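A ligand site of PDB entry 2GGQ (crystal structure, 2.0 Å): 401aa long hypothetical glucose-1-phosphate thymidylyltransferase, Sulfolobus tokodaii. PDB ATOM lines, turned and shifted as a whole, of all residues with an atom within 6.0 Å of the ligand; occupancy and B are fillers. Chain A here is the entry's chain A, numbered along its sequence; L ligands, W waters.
The side-chain amino group (NZ) of Lys 23 lies within salt-bridge range of the side-chain carboxylate (OD2) of Asp 99 (2.8 Å).
OE2 of Glu 181 lies within salt-bridge range of NH1 of Arg 179 (2.5 Å).
The side-chain amide oxygen (OE1) of Gln 73 lies close to the backbone NH (N) of Ala 83.
O of Ile 77 lies within hydrogen-bond range of NE2 of Gln 73, 3.2 Å away.
OE1 of Glu 12 lies within salt-bridge range of NZ of Lys 344, 3.6 Å away.
N of Ala 8 is in hydrogen-bond range of O of Ile 52.
O of Leu 6 is in hydrogen-bond range of N of Gly 98 (2.8 Å).
O of Ile 52 lies within hydrogen-bond range of N of Ala 7, 2.9 Å away.
An oxygen (O5) of the ligand sits at hydrogen-bond distance from the backbone NH of Ser 10, at 3.4 Å.
An oxygen (O8) of the ligand is in hydrogen-bond range of the side-chain hydroxyl (OG) of Ser 10 (2.6 Å).
NZ of Lys 23 lies within salt-bridge range of O4 of the ligand, 2.7 Å away.
OE1 of Glu 181 is in hydrogen-bond range of O12 of the ligand (2.8 Å).
The backbone NH of Arg 13 lies within hydrogen-bond range of an oxygen (O7) of the ligand (3.1 Å).
O7 of the ligand is in salt-bridge range of NE of Arg 13.
The side-chain amide oxygen (OE1) of Gln 73 is in hydrogen-bond range of a nitrogen (N2) of the ligand (2.9 Å).
The backbone NH (N) of Gly 11 sits at hydrogen-bond distance from an oxygen (O4) of the ligand (2.9 Å).
An oxygen (O8) of the ligand is in salt-bridge range of the side-chain amino group (NZ) of Lys 344, 3.0 Å away.
The backbone NH (N) of Gly 79 sits at hydrogen-bond distance from an oxygen (O13) of the ligand, 3.0 Å away.
The backbone carbonyl oxygen (O) of Gly 79 lies within hydrogen-bond range of a nitrogen (N2) of the ligand.
An oxygen (O8) of the ligand lies within hydrogen-bond range of the backbone NH of Glu 12, 3.0 Å away.
An oxygen (O14) of the ligand sits at hydrogen-bond distance from the backbone NH of Ala 8 (3.2 Å).
O of Ala 8 lies close to N2 of the ligand (3.3 Å).
CB of Leu 6 touches O14 of the ligand, 3.5 Å away.
Ala 7 touches the ligand (N to O14, 3.8 Å).
Gly 9 touches the ligand (CA to O5, 3.0 Å).
Lys 78 touches the ligand (CD to O12, 3.7 Å).
Ala 83 touches the ligand (CB to O14, 3.2 Å).
Asp 99 touches the ligand (OD2 to O2, 3.9 Å).
NH2 of Arg 179 touches C1 of the ligand (3.3 Å).
Water W1 lies within hydrogen-bond range of an oxygen (O7) of the ligand (2.7 Å), the backbone carbonyl oxygen of Gly 210 (2.8 Å) and the side-chain amino group of Lys 23 (2.9 Å).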
ATOM      1  N   LEU A   6      13.691 -16.043 -29.521  1.00  0.00           N
ATOM      2  CA  LEU A   6      13.189 -17.093 -28.650  1.00  0.00           C
ATOM      3  C   LEU A   6      11.871 -16.568 -28.085  1.00  0.00           C
ATOM      4  O   LEU A   6      11.849 -15.706 -27.199  1.00  0.00           O
ATOM      5  CB  LEU A   6      14.166 -17.442 -27.547  1.00  0.00           C
ATOM      6  CG  LEU A   6      15.609 -17.688 -28.015  1.00  0.00           C
ATOM      7  CD1 LEU A   6      16.505 -18.029 -26.849  1.00  0.00           C
ATOM      8  CD2 LEU A   6      15.655 -18.767 -29.081  1.00  0.00           C
ATOM      9  N   ALA A   7      10.782 -17.054 -28.682  1.00  0.00           N
ATOM     10  CA  ALA A   7       9.439 -16.549 -28.412  1.00  0.00           C
ATOM     11  C   ALA A   7       8.491 -17.665 -27.960  1.00  0.00           C
ATOM     12  O   ALA A   7       7.277 -17.626 -28.257  1.00  0.00           O
ATOM     13  CB  ALA A   7       8.884 -15.858 -29.628  1.00  0.00           C
ATOM     14  N   ALA A   8       9.050 -18.668 -27.295  1.00  0.00           N
ATOM     15  CA  ALA A   8       8.275 -19.825 -26.866  1.00  0.00           C
ATOM     16  C   ALA A   8       8.058 -19.878 -25.340  1.00  0.00           C
ATOM     17  O   ALA A   8       7.812 -20.954 -24.771  1.00  0.00           O
ATOM     18  CB  ALA A   8       8.928 -21.102 -27.376  1.00  0.00           C
ATOM     19  N   GLY A   9       8.151 -18.728 -24.693  1.00  0.00           N
ATOM     20  CA  GLY A   9       7.856 -18.586 -23.263  1.00  0.00           C
ATOM     21  C   GLY A   9       6.356 -18.773 -23.043  1.00  0.00           C
ATOM     22  O   GLY A   9       5.547 -18.615 -23.965  1.00  0.00           O
ATOM     23  N   SER A  10       5.994 -19.130 -21.815  1.00  0.00           N
ATOM     24  CA  SER A  10       4.610 -19.402 -21.498  1.00  0.00           C
ATOM     25  C   SER A  10       3.747 -18.131 -21.330  1.00  0.00           C
ATOM     26  O   SER A  10       2.527 -18.219 -21.396  1.00  0.00           O
ATOM     27  CB  SER A  10       4.522 -20.280 -20.266  1.00  0.00           C
ATOM     28  OG  SER A  10       5.470 -19.857 -19.307  1.00  0.00           O
ATOM     29  N   GLY A  11       4.370 -16.983 -21.087  1.00  0.00           N
ATOM     30  CA  GLY A  11       3.608 -15.720 -20.994  1.00  0.00           C
ATOM     31  C   GLY A  11       2.498 -15.673 -19.936  1.00  0.00           C
ATOM     32  O   GLY A  11       1.586 -14.839 -20.020  1.00  0.00           O
ATOM     33  N   GLU A  12       2.587 -16.547 -18.932  1.00  0.00           N
ATOM     34  CA  GLU A  12       1.626 -16.552 -17.805  1.00  0.00           C
ATOM     35  C   GLU A  12       1.605 -15.286 -16.939  1.00  0.00           C
ATOM     36  O   GLU A  12       0.558 -14.864 -16.423  1.00  0.00           O
ATOM     37  CB  GLU A  12       1.835 -17.788 -16.915  1.00  0.00           C
ATOM     38  CG  GLU A  12       1.230 -19.035 -17.553  1.00  0.00           C
ATOM     39  CD  GLU A  12       1.767 -20.328 -16.979  1.00  0.00           C
ATOM     40  OE1 GLU A  12       1.873 -20.424 -15.736  1.00  0.00           O
ATOM     41  OE2 GLU A  12       2.084 -21.239 -17.789  1.00  0.00           O
ATOM     42  N   ARG A  13       2.775 -14.683 -16.724  1.00  0.00           N
ATOM     43  CA  ARG A  13       2.821 -13.439 -15.942  1.00  0.00           C
ATOM     44  C   ARG A  13       2.184 -12.255 -16.639  1.00  0.00           C
ATOM     45  O   ARG A  13       1.961 -11.205 -16.031  1.00  0.00           O
ATOM     46  CB  ARG A  13       4.266 -13.067 -15.592  1.00  0.00           C
ATOM     47  CG  ARG A  13       5.051 -14.111 -14.783  1.00  0.00           C
ATOM     48  CD  ARG A  13       6.536 -13.609 -14.634  1.00  0.00           C
ATOM     49  NE  ARG A  13       7.250 -13.683 -15.912  1.00  0.00           N
ATOM     50  CZ  ARG A  13       8.151 -12.797 -16.340  1.00  0.00           C
ATOM     51  NH1 ARG A  13       8.476 -11.715 -15.630  1.00  0.00           N
ATOM     52  NH2 ARG A  13       8.721 -12.987 -17.504  1.00  0.00           N
ATOM     53  N   LEU A  14       1.914 -12.412 -17.927  1.00  0.00           N
ATOM     54  CA  LEU A  14       1.338 -11.313 -18.693  1.00  0.00           C
ATOM     55  C   LEU A  14      -0.136 -11.519 -18.978  1.00  0.00           C
ATOM     56  O   LEU A  14      -0.732 -10.808 -19.774  1.00  0.00           O
ATOM     57  CB  LEU A  14       2.133 -11.079 -19.985  1.00  0.00           C
ATOM     58  CG  LEU A  14       1.988  -9.682 -20.586  1.00  0.00           C
ATOM     59  CD1 LEU A  14       2.671  -8.598 -19.764  1.00  0.00           C
ATOM     60  CD2 LEU A  14       2.439  -9.617 -22.031  1.00  0.00           C
ATOM     61  N   LYS A  23       2.993 -13.050 -26.342  1.00  0.00           N
ATOM     62  CA  LYS A  23       3.653 -11.866 -25.795  1.00  0.00           C
ATOM     63  C   LYS A  23       4.382 -11.058 -26.871  1.00  0.00           C
ATOM     64  O   LYS A  23       4.421  -9.815 -26.798  1.00  0.00           O
ATOM     65  CB  LYS A  23       4.533 -12.291 -24.608  1.00  0.00           C
ATOM     66  CG  LYS A  23       5.500 -11.269 -23.976  1.00  0.00           C
ATOM     67  CD  LYS A  23       5.886 -11.598 -22.466  1.00  0.00           C
ATOM     68  CE  LYS A  23       6.410 -13.015 -22.198  1.00  0.00           C
ATOM     69  NZ  LYS A  23       7.371 -13.031 -21.045  1.00  0.00           N
ATOM     70  N   ILE A  52      11.344 -18.900 -32.828  1.00  0.00           N
ATOM     71  CA  ILE A  52      11.027 -20.178 -32.209  1.00  0.00           C
ATOM     72  C   ILE A  52       9.790 -20.003 -31.281  1.00  0.00           C
ATOM     73  O   ILE A  52       9.803 -19.135 -30.408  1.00  0.00           O
ATOM     74  CB  ILE A  52      12.217 -20.673 -31.440  1.00  0.00           C
ATOM     75  CG1 ILE A  52      13.390 -20.918 -32.445  1.00  0.00           C
ATOM     76  CG2 ILE A  52      11.865 -21.929 -30.676  1.00  0.00           C
ATOM     77  CD1 ILE A  52      14.740 -20.958 -31.806  1.00  0.00           C
ATOM     78  N   GLN A  73       9.290 -25.038 -30.859  1.00  0.00           N
ATOM     79  CA  GLN A  73      10.133 -25.620 -29.847  1.00  0.00           C
ATOM     80  C   GLN A  73       9.696 -27.082 -29.614  1.00  0.00           C
ATOM     81  O   GLN A  73       8.515 -27.394 -29.732  1.00  0.00           O
ATOM     82  CB  GLN A  73       9.981 -24.823 -28.564  1.00  0.00           C
ATOM     83  CG  GLN A  73      10.725 -25.349 -27.371  1.00  0.00           C
ATOM     84  CD  GLN A  73      10.803 -24.356 -26.254  1.00  0.00           C
ATOM     85  OE1 GLN A  73      11.261 -23.231 -26.441  1.00  0.00           O
ATOM     86  NE2 GLN A  73      10.376 -24.760 -25.075  1.00  0.00           N
ATOM     87  N   ILE A  77      10.175 -30.450 -23.842  1.00  0.00           N
ATOM     88  CA  ILE A  77      11.200 -29.712 -23.102  1.00  0.00           C
ATOM     89  C   ILE A  77      10.854 -28.231 -22.933  1.00  0.00           C
ATOM     90  O   ILE A  77      10.134 -27.642 -23.762  1.00  0.00           O
ATOM     91  CB  ILE A  77      12.635 -29.870 -23.741  1.00  0.00           C
ATOM     92  CG1 ILE A  77      12.576 -29.820 -25.270  1.00  0.00           C
ATOM     93  CG2 ILE A  77      13.311 -31.145 -23.243  1.00  0.00           C
ATOM     94  CD1 ILE A  77      13.941 -29.750 -25.962  1.00  0.00           C
ATOM     95  N   LYS A  78      11.354 -27.620 -21.848  1.00  0.00           N
ATOM     96  CA  LYS A  78      11.148 -26.182 -21.651  1.00  0.00           C
ATOM     97  C   LYS A  78      12.436 -25.430 -21.324  1.00  0.00           C
ATOM     98  O   LYS A  78      13.405 -26.022 -20.820  1.00  0.00           O
ATOM     99  CB  LYS A  78      10.085 -25.910 -20.574  1.00  0.00           C
ATOM    100  CG  LYS A  78      10.550 -26.167 -19.160  1.00  0.00           C
ATOM    101  CD  LYS A  78       9.585 -25.602 -18.126  1.00  0.00           C
ATOM    102  CE  LYS A  78       8.564 -26.644 -17.657  1.00  0.00           C
ATOM    103  NZ  LYS A  78       8.162 -26.406 -16.243  1.00  0.00           N
ATOM    104  N   GLY A  79      12.431 -24.125 -21.597  1.00  0.00           N
ATOM    105  CA  GLY A  79      13.521 -23.241 -21.192  1.00  0.00           C
ATOM    106  C   GLY A  79      14.144 -22.541 -22.373  1.00  0.00           C
ATOM    107  O   GLY A  79      13.878 -22.903 -23.524  1.00  0.00           O
ATOM    108  N   THR A  80      14.944 -21.523 -22.100  1.00  0.00           N
ATOM    109  CA  THR A  80      15.686 -20.815 -23.149  1.00  0.00           C
ATOM    110  C   THR A  80      16.634 -21.764 -23.882  1.00  0.00           C
ATOM    111  O   THR A  80      16.813 -21.650 -25.083  1.00  0.00           O
ATOM    112  CB  THR A  80      16.461 -19.636 -22.568  1.00  0.00           C
ATOM    113  OG1 THR A  80      17.266 -20.082 -21.466  1.00  0.00           O
ATOM    114  CG2 THR A  80      15.511 -18.536 -22.089  1.00  0.00           C
ATOM    115  N   ALA A  82      16.074 -25.052 -24.347  1.00  0.00           N
ATOM    116  CA  ALA A  82      15.265 -25.927 -25.214  1.00  0.00           C
ATOM    117  C   ALA A  82      14.880 -25.203 -26.510  1.00  0.00           C
ATOM    118  O   ALA A  82      14.770 -25.795 -27.597  1.00  0.00           O
ATOM    119  CB  ALA A  82      14.021 -26.407 -24.485  1.00  0.00           C
ATOM    120  N   ALA A  83      14.642 -23.897 -26.373  1.00  0.00           N
ATOM    121  CA  ALA A  83      14.316 -23.092 -27.515  1.00  0.00           C
ATOM    122  C   ALA A  83      15.469 -23.118 -28.547  1.00  0.00           C
ATOM    123  O   ALA A  83      15.222 -23.341 -29.729  1.00  0.00           O
ATOM    124  CB  ALA A  83      13.957 -21.650 -27.071  1.00  0.00           C
ATOM    125  N   TYR A  97      15.729 -12.590 -26.956  1.00  0.00           N
ATOM    126  CA  TYR A  97      14.503 -13.026 -26.279  1.00  0.00           C
ATOM    127  C   TYR A  97      13.311 -12.275 -26.827  1.00  0.00           C
ATOM    128  O   TYR A  97      13.389 -11.080 -27.061  1.00  0.00           O
ATOM    129  CB  TYR A  97      14.600 -12.841 -24.771  1.00  0.00           C
ATOM    130  CG  TYR A  97      15.603 -13.704 -24.070  1.00  0.00           C
ATOM    131  CD1 TYR A  97      16.062 -14.887 -24.645  1.00  0.00           C
ATOM    132  CD2 TYR A  97      16.050 -13.370 -22.792  1.00  0.00           C
ATOM    133  CE1 TYR A  97      16.994 -15.695 -23.997  1.00  0.00           C
ATOM    134  CE2 TYR A  97      16.988 -14.184 -22.118  1.00  0.00           C
ATOM    135  CZ  TYR A  97      17.444 -15.328 -22.728  1.00  0.00           C
ATOM    136  OH  TYR A  97      18.337 -16.147 -22.075  1.00  0.00           O
ATOM    137  N   GLY A  98      12.199 -12.980 -27.017  1.00  0.00           N
ATOM    138  CA  GLY A  98      11.041 -12.431 -27.706  1.00  0.00           C
ATOM    139  C   GLY A  98      10.123 -11.431 -26.997  1.00  0.00           C
ATOM    140  O   GLY A  98       9.149 -10.949 -27.591  1.00  0.00           O
ATOM    141  N   ASP A  99      10.446 -11.112 -25.749  1.00  0.00           N
ATOM    142  CA  ASP A  99       9.684 -10.117 -24.992  1.00  0.00           C
ATOM    143  C   ASP A  99      10.475  -8.842 -24.630  1.00  0.00           C
ATOM    144  O   ASP A  99      10.079  -8.058 -23.743  1.00  0.00           O
ATOM    145  CB  ASP A  99       9.095 -10.755 -23.737  1.00  0.00           C
ATOM    146  CG  ASP A  99      10.162 -11.274 -22.764  1.00  0.00           C
ATOM    147  OD1 ASP A  99      11.384 -11.201 -23.027  1.00  0.00           O
ATOM    148  OD2 ASP A  99       9.731 -11.745 -21.703  1.00  0.00           O
ATOM    149  N   LYS A 147      19.026 -15.026 -10.802  1.00  0.00           N
ATOM    150  CA  LYS A 147      18.112 -14.559  -9.741  1.00  0.00           C
ATOM    151  C   LYS A 147      18.679 -14.721  -8.319  1.00  0.00           C
ATOM    152  O   LYS A 147      18.106 -15.437  -7.499  1.00  0.00           O
ATOM    153  CB  LYS A 147      16.731 -15.230  -9.869  1.00  0.00           C
ATOM    154  CG  LYS A 147      15.882 -14.657 -10.992  1.00  0.00           C
ATOM    155  CD  LYS A 147      14.410 -15.024 -10.856  1.00  0.00           C
ATOM    156  CE  LYS A 147      14.038 -16.201 -11.733  1.00  0.00           C
ATOM    157  NZ  LYS A 147      12.585 -16.188 -12.098  1.00  0.00           N
ATOM    158  N   ARG A 179      14.346 -26.011 -12.066  1.00  0.00           N
ATOM    159  CA  ARG A 179      13.110 -25.390 -12.531  1.00  0.00           C
ATOM    160  C   ARG A 179      12.337 -26.337 -13.458  1.00  0.00           C
ATOM    161  O   ARG A 179      11.224 -25.995 -13.915  1.00  0.00           O
ATOM    162  CB  ARG A 179      13.437 -24.053 -13.219  1.00  0.00           C
ATOM    163  CG  ARG A 179      12.328 -23.007 -13.208  1.00  0.00           C
ATOM    164  CD  ARG A 179      12.860 -21.629 -13.626  1.00  0.00           C
ATOM    165  NE  ARG A 179      11.771 -20.711 -13.995  1.00  0.00           N
ATOM    166  CZ  ARG A 179      11.738 -19.958 -15.097  1.00  0.00           C
ATOM    167  NH1 ARG A 179      12.750 -19.953 -15.960  1.00  0.00           N
ATOM    168  NH2 ARG A 179      10.687 -19.167 -15.317  1.00  0.00           N
ATOM    169  N   GLU A 181      13.820 -27.473 -16.265  1.00  0.00           N
ATOM    170  CA  GLU A 181      14.013 -26.594 -17.392  1.00  0.00           C
ATOM    171  C   GLU A 181      15.435 -26.654 -17.948  1.00  0.00           C
ATOM    172  O   GLU A 181      16.385 -26.788 -17.174  1.00  0.00           O
ATOM    173  CB  GLU A 181      13.750 -25.190 -16.881  1.00  0.00           C
ATOM    174  CG  GLU A 181      13.130 -24.281 -17.865  1.00  0.00           C
ATOM    175  CD  GLU A 181      12.563 -23.060 -17.215  1.00  0.00           C
ATOM    176  OE1 GLU A 181      11.437 -23.146 -16.672  1.00  0.00           O
ATOM    177  OE2 GLU A 181      13.243 -22.015 -17.244  1.00  0.00           O
ATOM    178  N   GLY A 210       7.400  -8.307 -18.913  1.00  0.00           N
ATOM    179  CA  GLY A 210       7.230  -9.504 -18.091  1.00  0.00           C
ATOM    180  C   GLY A 210       5.833  -9.486 -17.499  1.00  0.00           C
ATOM    181  O   GLY A 210       5.091 -10.483 -17.595  1.00  0.00           O
ATOM    182  N   LYS A 344       0.847 -15.258 -11.626  1.00  0.00           N
ATOM    183  CA  LYS A 344       1.195 -16.693 -11.540  1.00  0.00           C
ATOM    184  C   LYS A 344       0.988 -17.241 -10.136  1.00  0.00           C
ATOM    185  O   LYS A 344       1.874 -17.921  -9.591  1.00  0.00           O
ATOM    186  CB  LYS A 344       2.647 -16.924 -11.970  1.00  0.00           C
ATOM    187  CG  LYS A 344       2.836 -17.207 -13.418  1.00  0.00           C
ATOM    188  CD  LYS A 344       4.310 -17.504 -13.742  1.00  0.00           C
ATOM    189  CE  LYS A 344       4.586 -18.984 -13.837  1.00  0.00           C
ATOM    190  NZ  LYS A 344       5.214 -19.324 -15.151  1.00  0.00           N
HETATM  191  P1  LIG L   1      10.597 -15.727 -19.046  1.00  0.00           P
HETATM  192  O1  LIG L   1      11.119 -15.583 -17.620  1.00  0.00           O
HETATM  193  O2  LIG L   1      11.413 -14.850 -20.005  1.00  0.00           O
HETATM  194  O3  LIG L   1       9.016 -15.252 -19.126  1.00  0.00           O
HETATM  195  P2  LIG L   1       7.910 -16.230 -19.786  1.00  0.00           P
HETATM  196  O4  LIG L   1       6.896 -15.640 -20.717  1.00  0.00           O
HETATM  197  O5  LIG L   1       8.593 -17.267 -20.640  1.00  0.00           O
HETATM  198  O6  LIG L   1       7.355 -17.059 -18.543  1.00  0.00           O
HETATM  199  P3  LIG L   1       6.119 -16.722 -17.594  1.00  0.00           P
HETATM  200  O7  LIG L   1       5.539 -15.363 -17.937  1.00  0.00           O
HETATM  201  O8  LIG L   1       5.063 -17.804 -17.711  1.00  0.00           O
HETATM  202  O9  LIG L   1       6.722 -16.818 -16.209  1.00  0.00           O
HETATM  203  O10 LIG L   1      10.591 -17.308 -19.431  1.00  0.00           O
HETATM  204  C1  LIG L   1      10.155 -18.286 -18.446  1.00  0.00           C
HETATM  205  C2  LIG L   1       9.502 -19.604 -18.929  1.00  0.00           C
HETATM  206  O11 LIG L   1       9.345 -19.821 -20.350  1.00  0.00           O
HETATM  207  C3  LIG L   1      10.415 -20.736 -18.528  1.00  0.00           C
HETATM  208  O12 LIG L   1       9.584 -21.875 -18.260  1.00  0.00           O
HETATM  209  C4  LIG L   1      11.305 -20.974 -19.754  1.00  0.00           C
HETATM  210  C5  LIG L   1      10.297 -20.802 -20.876  1.00  0.00           C
HETATM  211  N1  LIG L   1      10.776 -20.424 -22.249  1.00  0.00           N
HETATM  212  C6  LIG L   1      10.741 -21.390 -23.317  1.00  0.00           C
HETATM  213  O13 LIG L   1      10.374 -22.584 -23.135  1.00  0.00           O
HETATM  214  N2  LIG L   1      11.107 -21.059 -24.560  1.00  0.00           N
HETATM  215  C7  LIG L   1      11.501 -19.821 -24.841  1.00  0.00           C
HETATM  216  O14 LIG L   1      11.814 -19.565 -26.015  1.00  0.00           O
HETATM  217  C8  LIG L   1      11.556 -18.791 -23.785  1.00  0.00           C
HETATM  218  C9  LIG L   1      11.996 -17.389 -24.090  1.00  0.00           C
HETATM  219  C10 LIG L   1      11.171 -19.166 -22.490  1.00  0.00           C
HETATM  220  O   HOH W   1       5.276 -12.909 -19.030  1.00  0.00           O
